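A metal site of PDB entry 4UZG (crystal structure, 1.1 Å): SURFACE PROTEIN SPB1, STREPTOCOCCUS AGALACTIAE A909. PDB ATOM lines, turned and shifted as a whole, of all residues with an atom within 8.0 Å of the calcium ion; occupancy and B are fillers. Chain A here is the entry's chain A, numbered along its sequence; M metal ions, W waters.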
ATOM      1  N   SER A  12     -17.957 -17.179 -19.394  1.00  0.00           N
ATOM      2  CA  SER A  12     -18.327 -17.012 -20.793  1.00  0.00           C
ATOM      3  C   SER A  12     -19.175 -18.191 -21.236  1.00  0.00           C
ATOM      4  O   SER A  12     -19.016 -19.318 -20.763  1.00  0.00           O
ATOM      5  CB  SER A  12     -17.100 -16.938 -21.712  1.00  0.00           C
ATOM      6  OG  SER A  12     -16.421 -15.707 -21.548  1.00  0.00           O
ATOM      7  N   VAL A  13     -20.091 -17.924 -22.179  1.00  0.00           N
ATOM      8  CA  VAL A  13     -20.843 -18.972 -22.826  1.00  0.00           C
ATOM      9  C   VAL A  13     -19.892 -20.047 -23.349  1.00  0.00           C
ATOM     10  O   VAL A  13     -18.852 -19.737 -23.945  1.00  0.00           O
ATOM     11  CB  VAL A  13     -21.743 -18.359 -23.912  1.00  0.00           C
ATOM     12  CG1 VAL A  13     -22.293 -19.425 -24.851  1.00  0.00           C
ATOM     13  CG2 VAL A  13     -22.881 -17.575 -23.263  1.00  0.00           C
ATOM     14  N   GLY A  14     -20.228 -21.298 -23.072  1.00  0.00           N
ATOM     15  CA  GLY A  14     -19.399 -22.447 -23.389  1.00  0.00           C
ATOM     16  C   GLY A  14     -18.510 -22.951 -22.257  1.00  0.00           C
ATOM     17  O   GLY A  14     -17.973 -24.059 -22.353  1.00  0.00           O
ATOM     18  N   ASP A  15     -18.361 -22.151 -21.218  1.00  0.00           N
ATOM     19  CA  ASP A  15     -17.512 -22.540 -20.097  1.00  0.00           C
ATOM     20  C   ASP A  15     -18.152 -23.681 -19.287  1.00  0.00           C
ATOM     21  O   ASP A  15     -19.376 -23.831 -19.206  1.00  0.00           O
ATOM     22  CB  ASP A  15     -17.281 -21.382 -19.113  1.00  0.00           C
ATOM     23  CG  ASP A  15     -16.309 -20.322 -19.599  1.00  0.00           C
ATOM     24  OD1 ASP A  15     -15.714 -20.444 -20.684  1.00  0.00           O
ATOM     25  OD2 ASP A  15     -16.160 -19.350 -18.823  1.00  0.00           O
ATOM     26  N   THR A  16     -17.286 -24.460 -18.675  1.00  0.00           N
ATOM     27  CA  THR A  16     -17.679 -25.439 -17.668  1.00  0.00           C
ATOM     28  C   THR A  16     -17.914 -24.722 -16.345  1.00  0.00           C
ATOM     29  O   THR A  16     -17.031 -24.010 -15.841  1.00  0.00           O
ATOM     30  CB  THR A  16     -16.591 -26.495 -17.499  1.00  0.00           C
ATOM     31  OG1 THR A  16     -16.409 -27.143 -18.757  1.00  0.00           O
ATOM     32  CG2 THR A  16     -16.981 -27.526 -16.444  1.00  0.00           C
ATOM     33  N   VAL A 130     -22.474 -26.914 -18.544  1.00  0.00           N
ATOM     34  CA  VAL A 130     -21.891 -26.037 -19.556  1.00  0.00           C
ATOM     35  C   VAL A 130     -22.844 -24.886 -19.838  1.00  0.00           C
ATOM     36  O   VAL A 130     -24.026 -25.098 -20.127  1.00  0.00           O
ATOM     37  CB  VAL A 130     -21.557 -26.814 -20.850  1.00  0.00           C
ATOM     38  CG1 VAL A 130     -21.043 -25.878 -21.934  1.00  0.00           C
ATOM     39  CG2 VAL A 130     -20.546 -27.931 -20.573  1.00  0.00           C
ATOM     40  N   ASN A 200     -13.775 -15.795 -31.274  1.00  0.00           N
ATOM     41  CA  ASN A 200     -14.541 -16.528 -32.264  1.00  0.00           C
ATOM     42  C   ASN A 200     -15.803 -17.004 -31.545  1.00  0.00           C
ATOM     43  O   ASN A 200     -15.726 -17.805 -30.603  1.00  0.00           O
ATOM     44  CB  ASN A 200     -13.774 -17.714 -32.831  1.00  0.00           C
ATOM     45  CG  ASN A 200     -14.650 -18.513 -33.806  1.00  0.00           C
ATOM     46  OD1 ASN A 200     -15.761 -18.911 -33.512  1.00  0.00           O
ATOM     47  ND2 ASN A 200     -14.175 -18.658 -35.022  1.00  0.00           N
ATOM     48  N   ASN A 205     -23.092 -21.341 -28.944  1.00  0.00           N
ATOM     49  CA  ASN A 205     -23.021 -21.889 -27.589  1.00  0.00           C
ATOM     50  C   ASN A 205     -21.603 -21.972 -27.029  1.00  0.00           C
ATOM     51  O   ASN A 205     -21.430 -22.571 -25.963  1.00  0.00           O
ATOM     52  CB  ASN A 205     -23.694 -23.249 -27.531  1.00  0.00           C
ATOM     53  CG  ASN A 205     -25.169 -23.158 -27.767  1.00  0.00           C
ATOM     54  OD1 ASN A 205     -25.884 -22.468 -27.026  1.00  0.00           O
ATOM     55  ND2 ASN A 205     -25.643 -23.825 -28.832  1.00  0.00           N
ATOM     56  N   ASN A 206     -20.603 -21.372 -27.679  1.00  0.00           N
ATOM     57  CA  ASN A 206     -19.258 -21.510 -27.179  1.00  0.00           C
ATOM     58  C   ASN A 206     -18.336 -20.391 -27.615  1.00  0.00           C
ATOM     59  O   ASN A 206     -17.834 -20.378 -28.747  1.00  0.00           O
ATOM     60  CB  ASN A 206     -18.663 -22.861 -27.588  1.00  0.00           C
ATOM     61  CG  ASN A 206     -17.298 -23.070 -26.984  1.00  0.00           C
ATOM     62  OD1 ASN A 206     -16.973 -22.518 -25.928  1.00  0.00           O
ATOM     63  ND2 ASN A 206     -16.513 -23.901 -27.616  1.00  0.00           N
ATOM     64  N   VAL A 207     -18.065 -19.436 -26.715  1.00  0.00           N
ATOM     65  CA  VAL A 207     -17.005 -18.458 -26.897  1.00  0.00           C
ATOM     66  C   VAL A 207     -15.672 -19.164 -27.013  1.00  0.00           C
ATOM     67  O   VAL A 207     -15.357 -20.011 -26.172  1.00  0.00           O
ATOM     68  CB  VAL A 207     -16.982 -17.518 -25.658  1.00  0.00           C
ATOM     69  CG1 VAL A 207     -15.675 -16.731 -25.529  1.00  0.00           C
ATOM     70  CG2 VAL A 207     -18.188 -16.586 -25.644  1.00  0.00           C
ATOM     71  N   GLU A 208     -14.870 -18.791 -28.018  1.00  0.00           N
ATOM     72  CA  GLU A 208     -13.527 -19.309 -28.162  1.00  0.00           C
ATOM     73  C   GLU A 208     -12.578 -18.149 -28.411  1.00  0.00           C
ATOM     74  O   GLU A 208     -12.965 -17.092 -28.935  1.00  0.00           O
ATOM     75  CB  GLU A 208     -13.454 -20.303 -29.315  1.00  0.00           C
ATOM     76  CG  GLU A 208     -14.063 -21.678 -28.958  1.00  0.00           C
ATOM     77  CD  GLU A 208     -13.209 -22.433 -27.929  1.00  0.00           C
ATOM     78  OE1 GLU A 208     -11.989 -22.667 -28.186  1.00  0.00           O
ATOM     79  OE2 GLU A 208     -13.671 -22.692 -26.819  1.00  0.00           O
ATOM     80  N   TRP A 209     -11.322 -18.354 -28.036  1.00  0.00           N
ATOM     81  CA  TRP A 209     -10.271 -17.350 -28.133  1.00  0.00           C
ATOM     82  C   TRP A 209      -9.137 -17.924 -28.964  1.00  0.00           C
ATOM     83  O   TRP A 209      -8.660 -19.016 -28.680  1.00  0.00           O
ATOM     84  CB  TRP A 209      -9.787 -16.948 -26.745  1.00  0.00           C
ATOM     85  CG  TRP A 209     -10.852 -16.328 -25.917  1.00  0.00           C
ATOM     86  CD1 TRP A 209     -11.541 -16.921 -24.896  1.00  0.00           C
ATOM     87  CD2 TRP A 209     -11.409 -15.021 -26.082  1.00  0.00           C
ATOM     88  NE1 TRP A 209     -12.492 -16.071 -24.417  1.00  0.00           N
ATOM     89  CE2 TRP A 209     -12.430 -14.888 -25.115  1.00  0.00           C
ATOM     90  CE3 TRP A 209     -11.124 -13.938 -26.926  1.00  0.00           C
ATOM     91  CZ2 TRP A 209     -13.176 -13.725 -24.986  1.00  0.00           C
ATOM     92  CZ3 TRP A 209     -11.850 -12.802 -26.798  1.00  0.00           C
ATOM     93  CH2 TRP A 209     -12.873 -12.689 -25.839  1.00  0.00           C
HETATM   94 CA    CA M   1     -14.899 -21.907 -24.885  1.00  0.00          CA
HETATM   95  O   HOH W   1     -14.195 -22.561 -22.546  1.00  0.00           O
HETATM   96  O   HOH W   2     -14.928 -24.307 -24.691  1.00  0.00           O
HETATM   97  O   HOH W   3     -12.812 -20.852 -24.504  1.00  0.00           O
HETATM   98  O   HOH W   4     -16.315 -20.791 -23.368  1.00  0.00           O
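The backbone carbonyl oxygen (O) of Val 13 lies within hydrogen-bond range of the backbone NH (N) of Val 207, at 2.9 Å.
N of Asn 200 is in hydrogen-bond range of O of Glu 208 (2.8 Å).
Of the 12 residues printed, 3 come within 4 Å of the calcium ion.
The nearest printed residue that does not touch the calcium ion is Asp 15 (4.5 Å).
The calcium ion is bound by O of Val 207 (2.3 Å), water W4 (2.4 Å), water W3 (2.4 Å), OD1 of Asn 206 (2.4 Å), water W2 (2.4 Å), OE2 of Glu 208 (2.4 Å) and water W1 (2.5 Å).
Water W4 lies within hydrogen-bond range of the side-chain carboxylate of Asp 15 (2.8 Å) and the backbone carbonyl oxygen of Val 13 (2.8 Å).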
